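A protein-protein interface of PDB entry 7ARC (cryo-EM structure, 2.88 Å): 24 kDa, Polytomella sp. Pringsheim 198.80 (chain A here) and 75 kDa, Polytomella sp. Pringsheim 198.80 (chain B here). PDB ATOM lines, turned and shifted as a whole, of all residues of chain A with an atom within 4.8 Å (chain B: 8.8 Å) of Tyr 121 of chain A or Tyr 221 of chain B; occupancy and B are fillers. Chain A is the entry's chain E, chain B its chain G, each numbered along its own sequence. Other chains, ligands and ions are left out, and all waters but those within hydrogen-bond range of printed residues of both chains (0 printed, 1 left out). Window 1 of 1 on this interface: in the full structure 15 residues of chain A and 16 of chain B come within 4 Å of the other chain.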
ATOM      1  N   ASN A  46     -18.588  11.326  17.466  1.00  0.00           N
ATOM      2  CA  ASN A  46     -19.459  10.348  16.833  1.00  0.00           C
ATOM      3  C   ASN A  46     -19.855   9.241  17.800  1.00  0.00           C
ATOM      4  O   ASN A  46     -20.460   8.249  17.385  1.00  0.00           O
ATOM      5  CB  ASN A  46     -18.778   9.748  15.604  1.00  0.00           C
ATOM      6  CG  ASN A  46     -19.088  10.508  14.336  1.00  0.00           C
ATOM      7  OD1 ASN A  46     -20.226  10.905  14.098  1.00  0.00           O
ATOM      8  ND2 ASN A  46     -18.071  10.712  13.507  1.00  0.00           N
ATOM      9  N   VAL A  47     -19.514   9.393  19.079  1.00  0.00           N
ATOM     10  CA  VAL A  47     -19.910   8.483  20.142  1.00  0.00           C
ATOM     11  C   VAL A  47     -20.601   9.300  21.222  1.00  0.00           C
ATOM     12  O   VAL A  47     -20.476  10.524  21.283  1.00  0.00           O
ATOM     13  CB  VAL A  47     -18.714   7.708  20.734  1.00  0.00           C
ATOM     14  CG1 VAL A  47     -18.100   6.800  19.685  1.00  0.00           C
ATOM     15  CG2 VAL A  47     -17.681   8.673  21.284  1.00  0.00           C
ATOM     16  N   HIS A  48     -21.347   8.608  22.076  1.00  0.00           N
ATOM     17  CA  HIS A  48     -22.122   9.292  23.102  1.00  0.00           C
ATOM     18  C   HIS A  48     -21.192   9.876  24.158  1.00  0.00           C
ATOM     19  O   HIS A  48     -20.413   9.148  24.784  1.00  0.00           O
ATOM     20  CB  HIS A  48     -23.122   8.339  23.745  1.00  0.00           C
ATOM     21  CG  HIS A  48     -23.995   8.995  24.767  1.00  0.00           C
ATOM     22  ND1 HIS A  48     -24.847  10.033  24.462  1.00  0.00           N
ATOM     23  CD2 HIS A  48     -24.136   8.770  26.095  1.00  0.00           C
ATOM     24  CE1 HIS A  48     -25.481  10.415  25.555  1.00  0.00           C
ATOM     25  NE2 HIS A  48     -25.067   9.665  26.560  1.00  0.00           N
ATOM     26  N   LEU A 103     -29.942  11.064  23.860  1.00  0.00           N
ATOM     27  CA  LEU A 103     -29.988   9.609  23.928  1.00  0.00           C
ATOM     28  C   LEU A 103     -31.394   9.118  24.242  1.00  0.00           C
ATOM     29  O   LEU A 103     -31.835   8.091  23.715  1.00  0.00           O
ATOM     30  CB  LEU A 103     -29.000   9.098  24.973  1.00  0.00           C
ATOM     31  CG  LEU A 103     -28.518   7.669  24.747  1.00  0.00           C
ATOM     32  CD1 LEU A 103     -27.822   7.565  23.407  1.00  0.00           C
ATOM     33  CD2 LEU A 103     -27.603   7.235  25.875  1.00  0.00           C
ATOM     34  N   MET A 106     -33.415   9.154  21.008  1.00  0.00           N
ATOM     35  CA  MET A 106     -33.102   8.017  20.151  1.00  0.00           C
ATOM     36  C   MET A 106     -33.698   6.728  20.701  1.00  0.00           C
ATOM     37  O   MET A 106     -34.252   5.922  19.946  1.00  0.00           O
ATOM     38  CB  MET A 106     -31.590   7.887  19.980  1.00  0.00           C
ATOM     39  CG  MET A 106     -30.937   9.098  19.339  1.00  0.00           C
ATOM     40  SD  MET A 106     -29.190   8.840  18.988  1.00  0.00           S
ATOM     41  CE  MET A 106     -28.500  10.415  19.482  1.00  0.00           C
ATOM     42  N   ASN A 107     -33.597   6.518  22.015  1.00  0.00           N
ATOM     43  CA  ASN A 107     -34.159   5.308  22.603  1.00  0.00           C
ATOM     44  C   ASN A 107     -35.675   5.282  22.461  1.00  0.00           C
ATOM     45  O   ASN A 107     -36.258   4.225  22.198  1.00  0.00           O
ATOM     46  CB  ASN A 107     -33.755   5.199  24.072  1.00  0.00           C
ATOM     47  CG  ASN A 107     -32.298   4.832  24.249  1.00  0.00           C
ATOM     48  OD1 ASN A 107     -31.758   4.010  23.511  1.00  0.00           O
ATOM     49  ND2 ASN A 107     -31.654   5.434  25.238  1.00  0.00           N
ATOM     50  N   PRO A 117     -31.765  -0.254  19.029  1.00  0.00           N
ATOM     51  CA  PRO A 117     -31.387   1.165  19.124  1.00  0.00           C
ATOM     52  C   PRO A 117     -30.209   1.542  18.248  1.00  0.00           C
ATOM     53  O   PRO A 117     -30.049   2.728  17.937  1.00  0.00           O
ATOM     54  CB  PRO A 117     -31.069   1.341  20.614  1.00  0.00           C
ATOM     55  CG  PRO A 117     -30.727  -0.025  21.087  1.00  0.00           C
ATOM     56  CD  PRO A 117     -31.623  -0.945  20.319  1.00  0.00           C
ATOM     57  N   ILE A 118     -29.371   0.582  17.854  1.00  0.00           N
ATOM     58  CA  ILE A 118     -28.185   0.911  17.072  1.00  0.00           C
ATOM     59  C   ILE A 118     -28.576   1.474  15.712  1.00  0.00           C
ATOM     60  O   ILE A 118     -27.862   2.310  15.153  1.00  0.00           O
ATOM     61  CB  ILE A 118     -27.265  -0.318  16.937  1.00  0.00           C
ATOM     62  CG1 ILE A 118     -25.924   0.087  16.327  1.00  0.00           C
ATOM     63  CG2 ILE A 118     -27.919  -1.392  16.090  1.00  0.00           C
ATOM     64  CD1 ILE A 118     -25.098   0.978  17.211  1.00  0.00           C
ATOM     65  N   LYS A 119     -29.709   1.035  15.160  1.00  0.00           N
ATOM     66  CA  LYS A 119     -30.164   1.576  13.883  1.00  0.00           C
ATOM     67  C   LYS A 119     -30.492   3.059  14.004  1.00  0.00           C
ATOM     68  O   LYS A 119     -30.106   3.868  13.148  1.00  0.00           O
ATOM     69  CB  LYS A 119     -31.384   0.794  13.399  1.00  0.00           C
ATOM     70  CG  LYS A 119     -31.116  -0.682  13.158  1.00  0.00           C
ATOM     71  CD  LYS A 119     -30.174  -0.894  11.991  1.00  0.00           C
ATOM     72  CE  LYS A 119     -29.975  -2.372  11.709  1.00  0.00           C
ATOM     73  NZ  LYS A 119     -29.020  -2.594  10.591  1.00  0.00           N
ATOM     74  N   VAL A 120     -31.195   3.436  15.073  1.00  0.00           N
ATOM     75  CA  VAL A 120     -31.530   4.836  15.292  1.00  0.00           C
ATOM     76  C   VAL A 120     -30.276   5.640  15.599  1.00  0.00           C
ATOM     77  O   VAL A 120     -30.144   6.790  15.170  1.00  0.00           O
ATOM     78  CB  VAL A 120     -32.579   4.964  16.409  1.00  0.00           C
ATOM     79  CG1 VAL A 120     -32.954   6.416  16.621  1.00  0.00           C
ATOM     80  CG2 VAL A 120     -33.804   4.155  16.058  1.00  0.00           C
ATOM     81  N   TYR A 121     -29.328   5.046  16.327  1.00  0.00           N
ATOM     82  CA  TYR A 121     -28.052   5.714  16.565  1.00  0.00           C
ATOM     83  C   TYR A 121     -27.345   6.001  15.247  1.00  0.00           C
ATOM     84  O   TYR A 121     -26.851   7.112  15.015  1.00  0.00           O
ATOM     85  CB  TYR A 121     -27.164   4.851  17.462  1.00  0.00           C
ATOM     86  CG  TYR A 121     -27.689   4.637  18.863  1.00  0.00           C
ATOM     87  CD1 TYR A 121     -28.689   5.439  19.385  1.00  0.00           C
ATOM     88  CD2 TYR A 121     -27.179   3.625  19.663  1.00  0.00           C
ATOM     89  CE1 TYR A 121     -29.167   5.241  20.661  1.00  0.00           C
ATOM     90  CE2 TYR A 121     -27.650   3.420  20.940  1.00  0.00           C
ATOM     91  CZ  TYR A 121     -28.644   4.231  21.434  1.00  0.00           C
ATOM     92  OH  TYR A 121     -29.121   4.030  22.707  1.00  0.00           O
ATOM     93  N   GLU A 122     -27.312   5.007  14.359  1.00  0.00           N
ATOM     94  CA  GLU A 122     -26.628   5.154  13.082  1.00  0.00           C
ATOM     95  C   GLU A 122     -27.275   6.238  12.236  1.00  0.00           C
ATOM     96  O   GLU A 122     -26.581   7.065  11.635  1.00  0.00           O
ATOM     97  CB  GLU A 122     -26.647   3.825  12.330  1.00  0.00           C
ATOM     98  CG  GLU A 122     -25.549   2.859  12.712  1.00  0.00           C
ATOM     99  CD  GLU A 122     -25.614   1.568  11.917  1.00  0.00           C
ATOM    100  OE1 GLU A 122     -24.619   1.228  11.245  1.00  0.00           O
ATOM    101  OE2 GLU A 122     -26.662   0.890  11.964  1.00  0.00           O
ATOM    102  N   VAL A 123     -28.606   6.253  12.177  1.00  0.00           N
ATOM    103  CA  VAL A 123     -29.284   7.242  11.346  1.00  0.00           C
ATOM    104  C   VAL A 123     -29.164   8.640  11.948  1.00  0.00           C
ATOM    105  O   VAL A 123     -28.981   9.624  11.223  1.00  0.00           O
ATOM    106  CB  VAL A 123     -30.749   6.832  11.128  1.00  0.00           C
ATOM    107  CG1 VAL A 123     -31.496   7.901  10.359  1.00  0.00           C
ATOM    108  CG2 VAL A 123     -30.802   5.518  10.378  1.00  0.00           C
ATOM    109  N   ALA A 124     -29.253   8.756  13.276  1.00  0.00           N
ATOM    110  CA  ALA A 124     -29.086  10.053  13.923  1.00  0.00           C
ATOM    111  C   ALA A 124     -27.668  10.586  13.781  1.00  0.00           C
ATOM    112  O   ALA A 124     -27.459  11.802  13.807  1.00  0.00           O
ATOM    113  CB  ALA A 124     -29.465   9.953  15.399  1.00  0.00           C
ATOM    114  N   THR A 125     -26.687   9.701  13.631  1.00  0.00           N
ATOM    115  CA  THR A 125     -25.304  10.119  13.450  1.00  0.00           C
ATOM    116  C   THR A 125     -24.965  10.424  11.994  1.00  0.00           C
ATOM    117  O   THR A 125     -24.122  11.289  11.728  1.00  0.00           O
ATOM    118  CB  THR A 125     -24.373   9.036  13.999  1.00  0.00           C
ATOM    119  OG1 THR A 125     -24.646   8.840  15.389  1.00  0.00           O
ATOM    120  CG2 THR A 125     -22.936   9.448  13.862  1.00  0.00           C
ATOM    121  N   ARG A 132     -26.807  16.420  17.981  1.00  0.00           N
ATOM    122  CA  ARG A 132     -26.722  15.595  19.175  1.00  0.00           C
ATOM    123  C   ARG A 132     -26.078  16.320  20.347  1.00  0.00           C
ATOM    124  O   ARG A 132     -25.732  15.681  21.344  1.00  0.00           O
ATOM    125  CB  ARG A 132     -25.957  14.307  18.870  1.00  0.00           C
ATOM    126  CG  ARG A 132     -26.531  13.514  17.715  1.00  0.00           C
ATOM    127  CD  ARG A 132     -25.558  12.457  17.231  1.00  0.00           C
ATOM    128  NE  ARG A 132     -24.546  13.009  16.341  1.00  0.00           N
ATOM    129  CZ  ARG A 132     -23.249  13.041  16.609  1.00  0.00           C
ATOM    130  NH1 ARG A 132     -22.767  12.571  17.748  1.00  0.00           N
ATOM    131  NH2 ARG A 132     -22.413  13.557  15.712  1.00  0.00           N
ATOM    132  N   LYS B 175     -13.213   2.043  22.652  1.00  0.00           N
ATOM    133  CA  LYS B 175     -14.238   1.911  23.674  1.00  0.00           C
ATOM    134  C   LYS B 175     -14.339   0.458  24.112  1.00  0.00           C
ATOM    135  O   LYS B 175     -14.068  -0.462  23.338  1.00  0.00           O
ATOM    136  CB  LYS B 175     -15.601   2.384  23.161  1.00  0.00           C
ATOM    137  CG  LYS B 175     -15.696   3.875  22.909  1.00  0.00           C
ATOM    138  CD  LYS B 175     -17.053   4.236  22.329  1.00  0.00           C
ATOM    139  CE  LYS B 175     -18.154   4.092  23.364  1.00  0.00           C
ATOM    140  NZ  LYS B 175     -19.469   4.552  22.841  1.00  0.00           N
ATOM    141  N   LEU B 177     -15.783  -3.030  24.808  1.00  0.00           N
ATOM    142  CA  LEU B 177     -16.856  -3.908  24.359  1.00  0.00           C
ATOM    143  C   LEU B 177     -17.053  -5.108  25.272  1.00  0.00           C
ATOM    144  O   LEU B 177     -17.830  -6.007  24.936  1.00  0.00           O
ATOM    145  CB  LEU B 177     -16.614  -4.387  22.927  1.00  0.00           C
ATOM    146  CG  LEU B 177     -16.661  -3.354  21.806  1.00  0.00           C
ATOM    147  CD1 LEU B 177     -16.267  -3.993  20.494  1.00  0.00           C
ATOM    148  CD2 LEU B 177     -18.050  -2.760  21.707  1.00  0.00           C
ATOM    149  N   SER B 205     -27.407  -7.307  17.658  1.00  0.00           N
ATOM    150  CA  SER B 205     -27.603  -6.053  16.935  1.00  0.00           C
ATOM    151  C   SER B 205     -27.069  -4.864  17.727  1.00  0.00           C
ATOM    152  O   SER B 205     -27.758  -3.871  17.957  1.00  0.00           O
ATOM    153  CB  SER B 205     -29.078  -5.859  16.582  1.00  0.00           C
ATOM    154  OG  SER B 205     -29.523  -6.864  15.689  1.00  0.00           O
ATOM    155  N   GLU B 206     -25.822  -4.993  18.171  1.00  0.00           N
ATOM    156  CA  GLU B 206     -25.173  -3.988  19.002  1.00  0.00           C
ATOM    157  C   GLU B 206     -24.210  -3.102  18.230  1.00  0.00           C
ATOM    158  O   GLU B 206     -24.019  -1.943  18.608  1.00  0.00           O
ATOM    159  CB  GLU B 206     -24.431  -4.664  20.154  1.00  0.00           C
ATOM    160  CG  GLU B 206     -25.360  -5.333  21.143  1.00  0.00           C
ATOM    161  CD  GLU B 206     -24.605  -6.007  22.254  1.00  0.00           C
ATOM    162  OE1 GLU B 206     -23.364  -6.044  22.162  1.00  0.00           O
ATOM    163  OE2 GLU B 206     -25.242  -6.497  23.210  1.00  0.00           O
ATOM    164  N   LEU B 207     -23.599  -3.614  17.169  1.00  0.00           N
ATOM    165  CA  LEU B 207     -22.569  -2.903  16.426  1.00  0.00           C
ATOM    166  C   LEU B 207     -23.177  -2.288  15.175  1.00  0.00           C
ATOM    167  O   LEU B 207     -24.053  -2.880  14.540  1.00  0.00           O
ATOM    168  CB  LEU B 207     -21.415  -3.830  16.044  1.00  0.00           C
ATOM    169  CG  LEU B 207     -20.620  -4.438  17.195  1.00  0.00           C
ATOM    170  CD1 LEU B 207     -19.700  -5.524  16.682  1.00  0.00           C
ATOM    171  CD2 LEU B 207     -19.831  -3.370  17.919  1.00  0.00           C
ATOM    172  N   GLY B 208     -22.715  -1.090  14.835  1.00  0.00           N
ATOM    173  CA  GLY B 208     -23.149  -0.417  13.627  1.00  0.00           C
ATOM    174  C   GLY B 208     -22.114   0.597  13.204  1.00  0.00           C
ATOM    175  O   GLY B 208     -21.204   0.940  13.960  1.00  0.00           O
ATOM    176  N   ILE B 209     -22.254   1.064  11.967  1.00  0.00           N
ATOM    177  CA  ILE B 209     -21.366   2.087  11.428  1.00  0.00           C
ATOM    178  C   ILE B 209     -21.995   3.428  11.783  1.00  0.00           C
ATOM    179  O   ILE B 209     -22.950   3.867  11.144  1.00  0.00           O
ATOM    180  CB  ILE B 209     -21.204   1.947   9.912  1.00  0.00           C
ATOM    181  CG1 ILE B 209     -20.553   0.619   9.531  1.00  0.00           C
ATOM    182  CG2 ILE B 209     -20.365   3.092   9.370  1.00  0.00           C
ATOM    183  CD1 ILE B 209     -19.091   0.564   9.773  1.00  0.00           C
ATOM    184  N   THR B 210     -21.462   4.088  12.805  1.00  0.00           N
ATOM    185  CA  THR B 210     -21.902   5.427  13.169  1.00  0.00           C
ATOM    186  C   THR B 210     -20.949   6.452  12.572  1.00  0.00           C
ATOM    187  O   THR B 210     -19.737   6.383  12.796  1.00  0.00           O
ATOM    188  CB  THR B 210     -21.972   5.589  14.688  1.00  0.00           C
ATOM    189  OG1 THR B 210     -20.672   5.395  15.255  1.00  0.00           O
ATOM    190  CG2 THR B 210     -22.931   4.575  15.287  1.00  0.00           C
ATOM    191  N   GLY B 211     -21.494   7.396  11.816  1.00  0.00           N
ATOM    192  CA  GLY B 211     -20.705   8.419  11.170  1.00  0.00           C
ATOM    193  C   GLY B 211     -20.946   8.448   9.681  1.00  0.00           C
ATOM    194  O   GLY B 211     -21.666   7.626   9.118  1.00  0.00           O
ATOM    195  N   GLU B 217     -17.170   5.484  12.118  1.00  0.00           N
ATOM    196  CA  GLU B 217     -16.581   4.612  13.122  1.00  0.00           C
ATOM    197  C   GLU B 217     -17.497   3.433  13.405  1.00  0.00           C
ATOM    198  O   GLU B 217     -18.710   3.502  13.204  1.00  0.00           O
ATOM    199  CB  GLU B 217     -16.299   5.361  14.429  1.00  0.00           C
ATOM    200  CG  GLU B 217     -15.034   6.196  14.406  1.00  0.00           C
ATOM    201  CD  GLU B 217     -15.162   7.468  15.217  1.00  0.00           C
ATOM    202  OE1 GLU B 217     -16.305   7.882  15.491  1.00  0.00           O
ATOM    203  OE2 GLU B 217     -14.123   8.056  15.580  1.00  0.00           O
ATOM    204  N   VAL B 218     -16.891   2.344  13.869  1.00  0.00           N
ATOM    205  CA  VAL B 218     -17.580   1.091  14.147  1.00  0.00           C
ATOM    206  C   VAL B 218     -17.643   0.886  15.650  1.00  0.00           C
ATOM    207  O   VAL B 218     -16.658   1.114  16.362  1.00  0.00           O
ATOM    208  CB  VAL B 218     -16.862  -0.103  13.490  1.00  0.00           C
ATOM    209  CG1 VAL B 218     -17.650  -1.380  13.699  1.00  0.00           C
ATOM    210  CG2 VAL B 218     -16.597   0.160  12.033  1.00  0.00           C
ATOM    211  N   GLY B 219     -18.809   0.476  16.135  1.00  0.00           N
ATOM    212  CA  GLY B 219     -18.960   0.178  17.540  1.00  0.00           C
ATOM    213  C   GLY B 219     -20.308   0.579  18.088  1.00  0.00           C
ATOM    214  O   GLY B 219     -21.125   1.170  17.378  1.00  0.00           O
ATOM    215  N   THR B 220     -20.554   0.254  19.349  1.00  0.00           N
ATOM    216  CA  THR B 220     -21.758   0.724  20.013  1.00  0.00           C
ATOM    217  C   THR B 220     -21.657   2.230  20.204  1.00  0.00           C
ATOM    218  O   THR B 220     -20.621   2.739  20.642  1.00  0.00           O
ATOM    219  CB  THR B 220     -21.926   0.028  21.360  1.00  0.00           C
ATOM    220  OG1 THR B 220     -20.769   0.271  22.166  1.00  0.00           O
ATOM    221  CG2 THR B 220     -22.069  -1.465  21.166  1.00  0.00           C
ATOM    222  N   TYR B 221     -22.721   2.951  19.854  1.00  0.00           N
ATOM    223  CA  TYR B 221     -22.706   4.395  20.050  1.00  0.00           C
ATOM    224  C   TYR B 221     -22.659   4.746  21.532  1.00  0.00           C
ATOM    225  O   TYR B 221     -21.917   5.647  21.940  1.00  0.00           O
ATOM    226  CB  TYR B 221     -23.926   5.019  19.372  1.00  0.00           C
ATOM    227  CG  TYR B 221     -24.090   6.499  19.604  1.00  0.00           C
ATOM    228  CD1 TYR B 221     -23.360   7.420  18.868  1.00  0.00           C
ATOM    229  CD2 TYR B 221     -24.995   6.978  20.539  1.00  0.00           C
ATOM    230  CE1 TYR B 221     -23.513   8.773  19.069  1.00  0.00           C
ATOM    231  CE2 TYR B 221     -25.154   8.328  20.746  1.00  0.00           C
ATOM    232  CZ  TYR B 221     -24.412   9.221  20.008  1.00  0.00           C
ATOM    233  OH  TYR B 221     -24.568  10.572  20.214  1.00  0.00           O
ATOM    234  N   ILE B 222     -23.427   4.031  22.349  1.00  0.00           N
ATOM    235  CA  ILE B 222     -23.351   4.123  23.803  1.00  0.00           C
ATOM    236  C   ILE B 222     -22.230   3.226  24.304  1.00  0.00           C
ATOM    237  O   ILE B 222     -21.672   2.428  23.545  1.00  0.00           O
ATOM    238  CB  ILE B 222     -24.687   3.743  24.459  1.00  0.00           C
ATOM    239  CG1 ILE B 222     -25.012   2.280  24.172  1.00  0.00           C
ATOM    240  CG2 ILE B 222     -25.793   4.642  23.963  1.00  0.00           C
ATOM    241  CD1 ILE B 222     -26.168   1.755  24.975  1.00  0.00           C
ATOM    242  N   GLU B 223     -21.889   3.352  25.581  1.00  0.00           N
ATOM    243  CA  GLU B 223     -20.941   2.439  26.213  1.00  0.00           C
ATOM    244  C   GLU B 223     -21.699   1.165  26.561  1.00  0.00           C
ATOM    245  O   GLU B 223     -22.430   1.110  27.551  1.00  0.00           O
ATOM    246  CB  GLU B 223     -20.316   3.069  27.453  1.00  0.00           C
ATOM    247  CG  GLU B 223     -19.623   4.413  27.227  1.00  0.00           C
ATOM    248  CD  GLU B 223     -20.596   5.561  27.023  1.00  0.00           C
ATOM    249  OE1 GLU B 223     -21.676   5.548  27.651  1.00  0.00           O
ATOM    250  OE2 GLU B 223     -20.287   6.473  26.228  1.00  0.00           O
ATOM    251  N   LYS B 224     -21.529   0.135  25.735  1.00  0.00           N
ATOM    252  CA  LYS B 224     -22.189  -1.146  25.918  1.00  0.00           C
ATOM    253  C   LYS B 224     -21.177  -2.271  25.759  1.00  0.00           C
ATOM    254  O   LYS B 224     -20.168  -2.127  25.066  1.00  0.00           O
ATOM    255  CB  LYS B 224     -23.343  -1.334  24.914  1.00  0.00           C
ATOM    256  CG  LYS B 224     -24.173  -2.591  25.133  1.00  0.00           C
ATOM    257  CD  LYS B 224     -25.292  -2.722  24.118  1.00  0.00           C
ATOM    258  CE  LYS B 224     -26.387  -1.706  24.358  1.00  0.00           C
ATOM    259  NZ  LYS B 224     -27.111  -1.966  25.630  1.00  0.00           N
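Of the 16 printed residues of chain A, 9 touch a printed residue of chain B. Hydrophobic or aromatic side chains of chain A within 4 Å of the printed part of chain B: Val 47, His 48, Leu 103, Ile 118 and Tyr 121. Of the 17 printed residues of chain B, 13 touch a printed residue of chain A. Among the printed residues, no Asp or Glu carboxylate lies within 4 Å of a Lys or Arg side-chain nitrogen of the other chain.
The backbone carbonyl oxygen of Tyr 221 of chain B sits at hydrogen-bond distance from the backbone NH of His 48 of chain A (3.0 Å). The side-chain carboxylate (OE1) of Glu 122 of chain A sits at hydrogen-bond distance from the backbone NH (N) of Ile 209 of chain B (2.5 Å). The backbone carbonyl oxygen of His 48 of chain A sits close to the side-chain carboxylate of Glu 223 of chain B, at 3.0 Å.
Thr 210 of chain B touches Asn 46 of chain A (OG1 to O, 3.6 Å). Asn 46 of chain A touches Gly 211 of chain B (OD1 to CA, 3.9 Å). Lys 175 of chain B touches Val 47 of chain A. CD1 of Leu 103 of chain A touches CE2 of Tyr 221 of chain B, at 3.8 Å. Leu 103 of chain A touches Ile 222 of chain B. Ile 118 of chain A touches Gly 208 of chain B (CG1 to N, 3.7 Å). CD1 of Ile 118 of chain A touches O of Gly 219 of chain B (3.98 Å). OH of Tyr 121 of chain A touches CG2 of Ile 222 of chain B, at 3.6 Å. Thr 125 of chain A touches Gly 211 of chain B. CE1 of Tyr 221 of chain B touches OG1 of Thr 125 of chain A, 3.9 Å away.
Of the printed residues of chain A, Tyr 221 of chain B touches Asn 46, Val 47, His 48, Leu 103, Tyr 121, Thr 125 and Arg 132. No residue of chain B comes within 4 Å of Val 120 of chain A. Of the printed residues of chain B, Arg 132 of chain A touches Tyr 221. Printed residues of chain A within 4 Å of Thr 210 of chain B: Asn 46 and Thr 125. Printed residues of chain B within 4 Å of His 48 of chain A: Tyr 221 and Glu 223. Ala 124 of chain A touches none of the printed residues of chain B.
The side-chain amide nitrogen (ND2) of Asn 107 of chain A lies within hydrogen-bond range of the backbone carbonyl oxygen (O) of Leu 103 of chain A (3.1 Å). The backbone carbonyl oxygen of Tyr 121 of chain A lies within hydrogen-bond range of the side-chain hydroxyl of Thr 125 of chain A. NZ of Lys 175 of chain B sits at hydrogen-bond distance from O of Thr 220 of chain B, 3.1 Å away. O of Tyr 221 of chain B lies within hydrogen-bond range of NZ of Lys 175 of chain B (2.8 Å). NZ of Lys 175 of chain B is in salt-bridge range of OE2 of Glu 223 of chain B, 3.98 Å away. The backbone carbonyl oxygen (O) of Ile 222 of chain B sits at hydrogen-bond distance from the side-chain hydroxyl (OG1) of Thr 220 of chain B.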
